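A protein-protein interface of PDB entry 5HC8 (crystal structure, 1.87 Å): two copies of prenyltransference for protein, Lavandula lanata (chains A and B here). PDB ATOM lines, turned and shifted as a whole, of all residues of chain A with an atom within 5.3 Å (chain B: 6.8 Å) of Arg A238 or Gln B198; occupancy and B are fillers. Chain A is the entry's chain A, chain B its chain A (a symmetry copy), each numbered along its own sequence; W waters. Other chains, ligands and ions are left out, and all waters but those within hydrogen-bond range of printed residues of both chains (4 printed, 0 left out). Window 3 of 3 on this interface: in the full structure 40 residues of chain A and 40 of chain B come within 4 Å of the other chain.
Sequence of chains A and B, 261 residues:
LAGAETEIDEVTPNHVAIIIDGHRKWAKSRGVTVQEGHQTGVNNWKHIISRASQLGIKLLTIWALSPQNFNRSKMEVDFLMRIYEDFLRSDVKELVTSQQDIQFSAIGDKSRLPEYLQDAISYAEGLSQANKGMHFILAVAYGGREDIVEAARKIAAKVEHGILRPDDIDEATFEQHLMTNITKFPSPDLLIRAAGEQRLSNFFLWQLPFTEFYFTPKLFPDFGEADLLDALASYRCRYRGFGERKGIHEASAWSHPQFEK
OE2 of Glu A212 is in salt-bridge range of NH1 of Arg B199, at 2.7 Å. O of Gln B198 is in hydrogen-bond range of N of Phe A213, at 2.9 Å. NH1 of Arg B199 sits at hydrogen-bond distance from O of Tyr A239.
The side-chain carboxylate of Glu A212 lies within salt-bridge range of the guanidinium group of Arg A238 (2.8 Å). The backbone carbonyl oxygen of Phe A213 is in hydrogen-bond range of the guanidinium group of Arg A238 (2.8 Å). The side-chain hydroxyl (OG) of Ser A234 lies within hydrogen-bond range of the guanidinium group (NH2) of Arg A238 (3.0 Å). O of Arg B199 lies within hydrogen-bond range of NH1 of Arg B193, at 2.8 Å. NH1 of Arg B199 lies within salt-bridge range of OE2 of Glu B197, 3.3 Å away.
Among the printed residues, pairs that only touch across the chains: Thr A211 with Gln B198 (3.8 Å), Thr A211 with Arg B199 (3.2 Å), Glu A212 with Gln B198 (3.7 Å), Phe A213 with Leu B200 (3.7 Å), Phe A215 with Gln B198 (3.8 Å), Phe A215 with Phe B215 (3.6 Å), Arg A238 with Gln B198 (3.6 Å) and Tyr A239 with Glu B197 (3.7 Å).
Of chain B, only Gln B198 (3.6 Å) comes within 4 Å of Arg A238. Gln B198 touches just these residues of chain A: Thr A211 (3.8 Å), Glu A212 (3.7 Å), Phe A213 (2.9 Å), Phe A215 (3.8 Å) and Arg A238 (3.6 Å). Of the printed residues of chain B, Phe A215 touches Gln B198 and Phe B215. Of the printed residues of chain B, Phe A213 touches Gln B198 (2.9 Å) and Leu B200 (3.7 Å). Of the printed residues of chain A, Glu B197 touches Tyr A239. Printed residues of chain B within 4 Å of Thr A211: Gln B198 (3.8 Å) and Arg B199 (3.2 Å). Of the printed residues of chain B, Tyr A239 touches Glu B197 (3.7 Å) and Arg B199 (3.0 Å). The nearest residue of chain B that does not touch Arg A238 is Glu B197 (5.1 Å). The nearest residue of chain A that does not touch Gln B198 is Tyr A214 (5.1 Å).
Of the 12 printed residues of chain A, 6 touch a printed residue of chain B. Of the 7 printed residues of chain B, 5 touch a printed residue of chain A. Printed residues of chain B that touch a printed residue of chain A: Glu B197, Gln B198, Arg B199, Leu B200 and Phe B215. Among the printed residues, 11 pairs touch across the chains. Among the printed residues, Asp or Glu carboxylates within 4 Å of a Lys or Arg side-chain nitrogen of the other chain: Glu A212 with Arg B199 (2.7 Å).
Phe A215 touches its own counterpart, Phe B215. 1 position is printed for both chains. Of the 11 pairs that touch across the chains among the printed residues, 1 has its exchanged pair printed and touching as well.
Water W1 bridges O of Thr A211 (2.7 Å) and N of Leu B200 (2.8 Å). Water W4 lies within hydrogen-bond range of OE1 of Glu A212 (2.7 Å), N of Gln B198 (2.9 Å), OE2 of Glu B197 (2.9 Å) and NH1 of Arg A238 (3.5 Å). Water W3 lies within hydrogen-bond range of OE2 of Glu B197 (2.7 Å) and N of Tyr A239 (3.1 Å). Water W2 bridges the side-chain amide nitrogen of Gln B198 and the backbone NH of Phe A215.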
ATOM      1  N   THR A 211      20.996 -21.520 -11.065  1.00  0.00           N
ATOM      2  CA  THR A 211      20.890 -21.424  -9.641  1.00  0.00           C
ATOM      3  C   THR A 211      19.677 -22.177  -9.015  1.00  0.00           C
ATOM      4  O   THR A 211      18.546 -22.144  -9.500  1.00  0.00           O
ATOM      5  CB  THR A 211      20.734 -19.948  -9.302  1.00  0.00           C
ATOM      6  OG1 THR A 211      21.793 -19.210  -9.948  1.00  0.00           O
ATOM      7  CG2 THR A 211      20.726 -19.707  -7.808  1.00  0.00           C
ATOM      8  N   GLU A 212      19.959 -22.930  -7.960  1.00  0.00           N
ATOM      9  CA  GLU A 212      18.910 -23.556  -7.135  1.00  0.00           C
ATOM     10  C   GLU A 212      18.321 -22.498  -6.253  1.00  0.00           C
ATOM     11  O   GLU A 212      19.058 -21.762  -5.574  1.00  0.00           O
ATOM     12  CB  GLU A 212      19.548 -24.690  -6.309  1.00  0.00           C
ATOM     13  CG  GLU A 212      20.001 -25.847  -7.179  1.00  0.00           C
ATOM     14  CD  GLU A 212      18.849 -26.577  -7.858  1.00  0.00           C
ATOM     15  OE1 GLU A 212      17.748 -26.568  -7.323  1.00  0.00           O
ATOM     16  OE2 GLU A 212      19.038 -27.118  -8.942  1.00  0.00           O
ATOM     17  N   PHE A 213      16.997 -22.402  -6.238  1.00  0.00           N
ATOM     18  CA  PHE A 213      16.296 -21.484  -5.359  1.00  0.00           C
ATOM     19  C   PHE A 213      15.786 -22.199  -4.096  1.00  0.00           C
ATOM     20  O   PHE A 213      15.264 -23.323  -4.159  1.00  0.00           O
ATOM     21  CB  PHE A 213      15.087 -20.899  -6.072  1.00  0.00           C
ATOM     22  CG  PHE A 213      15.394 -20.124  -7.332  1.00  0.00           C
ATOM     23  CD1 PHE A 213      16.615 -19.551  -7.561  1.00  0.00           C
ATOM     24  CD2 PHE A 213      14.449 -19.988  -8.271  1.00  0.00           C
ATOM     25  CE1 PHE A 213      16.841 -18.785  -8.707  1.00  0.00           C
ATOM     26  CE2 PHE A 213      14.655 -19.245  -9.424  1.00  0.00           C
ATOM     27  CZ  PHE A 213      15.839 -18.609  -9.635  1.00  0.00           C
ATOM     28  N   TYR A 214      15.974 -21.547  -2.964  1.00  0.00           N
ATOM     29  CA  TYR A 214      15.460 -21.965  -1.709  1.00  0.00           C
ATOM     30  C   TYR A 214      14.705 -20.838  -1.028  1.00  0.00           C
ATOM     31  O   TYR A 214      15.243 -19.773  -0.767  1.00  0.00           O
ATOM     32  CB  TYR A 214      16.620 -22.401  -0.860  1.00  0.00           C
ATOM     33  CG  TYR A 214      16.261 -22.847   0.562  1.00  0.00           C
ATOM     34  CD1 TYR A 214      15.833 -24.129   0.827  1.00  0.00           C
ATOM     35  CD2 TYR A 214      16.329 -21.946   1.635  1.00  0.00           C
ATOM     36  CE1 TYR A 214      15.513 -24.530   2.114  1.00  0.00           C
ATOM     37  CE2 TYR A 214      15.997 -22.314   2.907  1.00  0.00           C
ATOM     38  CZ  TYR A 214      15.630 -23.595   3.161  1.00  0.00           C
ATOM     39  OH  TYR A 214      15.379 -23.936   4.454  1.00  0.00           O
ATOM     40  N   PHE A 215      13.428 -21.071  -0.768  1.00  0.00           N
ATOM     41  CA  PHE A 215      12.559 -20.076  -0.176  1.00  0.00           C
ATOM     42  C   PHE A 215      12.145 -20.552   1.210  1.00  0.00           C
ATOM     43  O   PHE A 215      11.702 -21.678   1.335  1.00  0.00           O
ATOM     44  CB  PHE A 215      11.333 -19.921  -1.044  1.00  0.00           C
ATOM     45  CG  PHE A 215      11.629 -19.504  -2.450  1.00  0.00           C
ATOM     46  CD1 PHE A 215      11.905 -18.211  -2.760  1.00  0.00           C
ATOM     47  CD2 PHE A 215      11.601 -20.455  -3.506  1.00  0.00           C
ATOM     48  CE1 PHE A 215      12.201 -17.832  -4.063  1.00  0.00           C
ATOM     49  CE2 PHE A 215      11.878 -20.037  -4.803  1.00  0.00           C
ATOM     50  CZ  PHE A 215      12.196 -18.746  -5.074  1.00  0.00           C
ATOM     51  N   SER A 234      19.047 -28.634   1.817  1.00  0.00           N
ATOM     52  CA  SER A 234      18.152 -28.722   0.669  1.00  0.00           C
ATOM     53  C   SER A 234      18.976 -28.795  -0.618  1.00  0.00           C
ATOM     54  O   SER A 234      18.672 -29.638  -1.521  1.00  0.00           O
ATOM     55  CB  SER A 234      17.123 -27.561   0.701  1.00  0.00           C
ATOM     56  OG  SER A 234      16.294 -27.461  -0.450  1.00  0.00           O
ATOM     57  N   TYR A 235      19.998 -27.910  -0.713  1.00  0.00           N
ATOM     58  CA  TYR A 235      20.919 -27.887  -1.824  1.00  0.00           C
ATOM     59  C   TYR A 235      21.526 -29.256  -2.107  1.00  0.00           C
ATOM     60  O   TYR A 235      21.509 -29.714  -3.232  1.00  0.00           O
ATOM     61  CB  TYR A 235      22.037 -26.886  -1.621  1.00  0.00           C
ATOM     62  CG  TYR A 235      22.972 -26.780  -2.780  1.00  0.00           C
ATOM     63  CD1 TYR A 235      22.591 -26.076  -3.949  1.00  0.00           C
ATOM     64  CD2 TYR A 235      24.220 -27.405  -2.769  1.00  0.00           C
ATOM     65  CE1 TYR A 235      23.411 -25.998  -5.001  1.00  0.00           C
ATOM     66  CE2 TYR A 235      25.060 -27.298  -3.852  1.00  0.00           C
ATOM     67  CZ  TYR A 235      24.640 -26.609  -4.948  1.00  0.00           C
ATOM     68  OH  TYR A 235      25.463 -26.511  -6.015  1.00  0.00           O
ATOM     69  N   ARG A 236      22.100 -29.878  -1.092  1.00  0.00           N
ATOM     70  CA  ARG A 236      22.720 -31.185  -1.304  1.00  0.00           C
ATOM     71  C   ARG A 236      21.722 -32.263  -1.767  1.00  0.00           C
ATOM     72  O   ARG A 236      22.096 -33.153  -2.502  1.00  0.00           O
ATOM     73  CB  ARG A 236      23.446 -31.651  -0.025  1.00  0.00           C
ATOM     74  CG  ARG A 236      24.616 -30.780   0.446  1.00  0.00           C
ATOM     75  CD  ARG A 236      25.317 -31.441   1.649  1.00  0.00           C
ATOM     76  NE  ARG A 236      25.640 -30.503   2.746  1.00  0.00           N
ATOM     77  CZ  ARG A 236      25.048 -30.445   3.959  1.00  0.00           C
ATOM     78  NH1 ARG A 236      24.063 -31.276   4.325  1.00  0.00           N
ATOM     79  NH2 ARG A 236      25.461 -29.534   4.842  1.00  0.00           N
ATOM     80  N   CYS A 237      20.469 -32.203  -1.336  1.00  0.00           N
ATOM     81  CA  CYS A 237      19.451 -33.059  -1.910  1.00  0.00           C
ATOM     82  C   CYS A 237      18.962 -32.687  -3.335  1.00  0.00           C
ATOM     83  O   CYS A 237      18.259 -33.451  -3.937  1.00  0.00           O
ATOM     84  CB  CYS A 237      18.255 -33.118  -0.982  1.00  0.00           C
ATOM     85  SG  CYS A 237      18.720 -33.792   0.607  1.00  0.00           S
ATOM     86  N   ARG A 238      19.335 -31.560  -3.909  1.00  0.00           N
ATOM     87  CA  ARG A 238      18.889 -31.264  -5.290  1.00  0.00           C
ATOM     88  C   ARG A 238      19.683 -32.074  -6.366  1.00  0.00           C
ATOM     89  O   ARG A 238      20.900 -32.227  -6.270  1.00  0.00           O
ATOM     90  CB  ARG A 238      19.080 -29.793  -5.658  1.00  0.00           C
ATOM     91  CG  ARG A 238      18.611 -28.720  -4.655  1.00  0.00           C
ATOM     92  CD  ARG A 238      17.130 -28.650  -4.661  1.00  0.00           C
ATOM     93  NE  ARG A 238      16.651 -27.720  -3.666  1.00  0.00           N
ATOM     94  CZ  ARG A 238      16.271 -26.459  -3.881  1.00  0.00           C
ATOM     95  NH1 ARG A 238      16.338 -25.855  -5.068  1.00  0.00           N
ATOM     96  NH2 ARG A 238      15.810 -25.786  -2.860  1.00  0.00           N
ATOM     97  N   TYR A 239      18.968 -32.534  -7.389  1.00  0.00           N
ATOM     98  CA  TYR A 239      19.574 -33.081  -8.615  1.00  0.00           C
ATOM     99  C   TYR A 239      19.624 -31.945  -9.632  1.00  0.00           C
ATOM    100  O   TYR A 239      18.568 -31.416  -9.981  1.00  0.00           O
ATOM    101  CB  TYR A 239      18.796 -34.284  -9.220  1.00  0.00           C
ATOM    102  CG  TYR A 239      19.416 -34.661 -10.558  1.00  0.00           C
ATOM    103  CD1 TYR A 239      20.626 -35.368 -10.614  1.00  0.00           C
ATOM    104  CD2 TYR A 239      18.848 -34.210 -11.769  1.00  0.00           C
ATOM    105  CE1 TYR A 239      21.226 -35.663 -11.832  1.00  0.00           C
ATOM    106  CE2 TYR A 239      19.440 -34.492 -12.990  1.00  0.00           C
ATOM    107  CZ  TYR A 239      20.624 -35.220 -13.022  1.00  0.00           C
ATOM    108  OH  TYR A 239      21.195 -35.484 -14.246  1.00  0.00           O
ATOM    109  N   ARG A 240      20.835 -31.589 -10.083  1.00  0.00           N
ATOM    110  CA  ARG A 240      21.061 -30.508 -11.084  1.00  0.00           C
ATOM    111  C   ARG A 240      21.401 -31.157 -12.441  1.00  0.00           C
ATOM    112  O   ARG A 240      22.422 -31.850 -12.585  1.00  0.00           O
ATOM    113  CB  ARG A 240      22.200 -29.558 -10.635  1.00  0.00           C
ATOM    114  CG  ARG A 240      22.247 -29.174  -9.123  1.00  0.00           C
ATOM    115  CD  ARG A 240      23.387 -28.177  -8.813  1.00  0.00           C
ATOM    116  NE  ARG A 240      23.115 -26.842  -9.399  1.00  0.00           N
ATOM    117  CZ  ARG A 240      23.937 -25.777  -9.368  1.00  0.00           C
ATOM    118  NH1 ARG A 240      25.169 -25.838  -8.826  1.00  0.00           N
ATOM    119  NH2 ARG A 240      23.542 -24.637  -9.910  1.00  0.00           N
ATOM    120  N   ARG B 193       6.358 -23.664 -12.866  1.00  0.00           N
ATOM    121  CA  ARG B 193       7.218 -24.777 -13.208  1.00  0.00           C
ATOM    122  C   ARG B 193       6.757 -26.055 -12.576  1.00  0.00           C
ATOM    123  O   ARG B 193       6.640 -26.147 -11.382  1.00  0.00           O
ATOM    124  CB  ARG B 193       8.687 -24.515 -12.850  1.00  0.00           C
ATOM    125  CG  ARG B 193       9.610 -25.693 -13.182  1.00  0.00           C
ATOM    126  CD  ARG B 193      11.092 -25.361 -13.058  1.00  0.00           C
ATOM    127  NE  ARG B 193      11.813 -26.576 -13.369  1.00  0.00           N
ATOM    128  CZ  ARG B 193      12.986 -26.635 -13.990  1.00  0.00           C
ATOM    129  NH1 ARG B 193      13.682 -25.550 -14.305  1.00  0.00           N
ATOM    130  NH2 ARG B 193      13.497 -27.810 -14.269  1.00  0.00           N
ATOM    131  N   GLY B 196       8.682 -30.017  -9.694  1.00  0.00           N
ATOM    132  CA  GLY B 196       9.220 -29.947  -8.348  1.00  0.00           C
ATOM    133  C   GLY B 196      10.577 -29.219  -8.268  1.00  0.00           C
ATOM    134  O   GLY B 196      10.992 -28.895  -7.166  1.00  0.00           O
ATOM    135  N   GLU B 197      11.292 -29.032  -9.392  1.00  0.00           N
ATOM    136  CA  GLU B 197      12.608 -28.358  -9.362  1.00  0.00           C
ATOM    137  C   GLU B 197      12.363 -26.868  -9.208  1.00  0.00           C
ATOM    138  O   GLU B 197      11.391 -26.309  -9.801  1.00  0.00           O
ATOM    139  CB  GLU B 197      13.484 -28.635 -10.580  1.00  0.00           C
ATOM    140  CG  GLU B 197      13.616 -30.126 -10.929  1.00  0.00           C
ATOM    141  CD  GLU B 197      14.403 -30.947  -9.910  1.00  0.00           C
ATOM    142  OE1 GLU B 197      14.284 -32.188  -9.996  1.00  0.00           O
ATOM    143  OE2 GLU B 197      15.109 -30.420  -9.026  1.00  0.00           O
ATOM    144  N   GLN B 198      13.272 -26.210  -8.485  1.00  0.00           N
ATOM    145  CA  GLN B 198      13.162 -24.793  -8.205  1.00  0.00           C
ATOM    146  C   GLN B 198      14.387 -24.066  -8.804  1.00  0.00           C
ATOM    147  O   GLN B 198      15.381 -23.840  -8.125  1.00  0.00           O
ATOM    148  CB  GLN B 198      13.059 -24.594  -6.693  1.00  0.00           C
ATOM    149  CG  GLN B 198      11.766 -25.147  -6.120  1.00  0.00           C
ATOM    150  CD  GLN B 198      11.851 -25.191  -4.590  1.00  0.00           C
ATOM    151  OE1 GLN B 198      12.428 -26.137  -3.970  1.00  0.00           O
ATOM    152  NE2 GLN B 198      11.424 -24.183  -4.004  1.00  0.00           N
ATOM    153  N   ARG B 199      14.257 -23.756 -10.089  1.00  0.00           N
ATOM    154  CA  ARG B 199      15.337 -23.165 -10.873  1.00  0.00           C
ATOM    155  C   ARG B 199      14.699 -22.813 -12.229  1.00  0.00           C
ATOM    156  O   ARG B 199      13.627 -23.306 -12.568  1.00  0.00           O
ATOM    157  CB  ARG B 199      16.555 -24.104 -11.054  1.00  0.00           C
ATOM    158  CG  ARG B 199      16.253 -25.449 -11.682  1.00  0.00           C
ATOM    159  CD  ARG B 199      17.512 -26.227 -12.008  1.00  0.00           C
ATOM    160  NE  ARG B 199      17.186 -27.583 -12.510  1.00  0.00           N
ATOM    161  CZ  ARG B 199      17.156 -28.700 -11.796  1.00  0.00           C
ATOM    162  NH1 ARG B 199      17.479 -28.712 -10.518  1.00  0.00           N
ATOM    163  NH2 ARG B 199      16.809 -29.841 -12.412  1.00  0.00           N
ATOM    164  N   LEU B 200      15.386 -21.942 -12.936  1.00  0.00           N
ATOM    165  CA  LEU B 200      14.963 -21.405 -14.227  1.00  0.00           C
ATOM    166  C   LEU B 200      15.477 -22.204 -15.384  1.00  0.00           C
ATOM    167  O   LEU B 200      14.871 -22.166 -16.476  1.00  0.00           O
ATOM    168  CB  LEU B 200      15.419 -19.937 -14.329  1.00  0.00           C
ATOM    169  CG  LEU B 200      14.897 -19.043 -13.185  1.00  0.00           C
ATOM    170  CD1 LEU B 200      15.545 -17.661 -13.342  1.00  0.00           C
ATOM    171  CD2 LEU B 200      13.378 -18.914 -13.225  1.00  0.00           C
ATOM    172  N   PHE B 215       5.816 -23.161  -8.026  1.00  0.00           N
ATOM    173  CA  PHE B 215       6.429 -24.452  -8.263  1.00  0.00           C
ATOM    174  C   PHE B 215       5.482 -25.539  -7.772  1.00  0.00           C
ATOM    175  O   PHE B 215       5.020 -25.451  -6.650  1.00  0.00           O
ATOM    176  CB  PHE B 215       7.725 -24.525  -7.493  1.00  0.00           C
ATOM    177  CG  PHE B 215       8.715 -23.465  -7.861  1.00  0.00           C
ATOM    178  CD1 PHE B 215       9.475 -23.567  -8.981  1.00  0.00           C
ATOM    179  CD2 PHE B 215       8.903 -22.331  -7.025  1.00  0.00           C
ATOM    180  CE1 PHE B 215      10.378 -22.570  -9.330  1.00  0.00           C
ATOM    181  CE2 PHE B 215       9.831 -21.363  -7.391  1.00  0.00           C
ATOM    182  CZ  PHE B 215      10.544 -21.472  -8.541  1.00  0.00           C
HETATM  183  O   HOH W   1      17.794 -21.009 -11.792  1.00  0.00           O
HETATM  184  O   HOH W   2      12.420 -23.686  -1.505  1.00  0.00           O
HETATM  185  O   HOH W   3      15.918 -32.097  -7.104  1.00  0.00           O
HETATM  186  O   HOH W   4      15.459 -27.877  -7.732  1.00  0.00           O
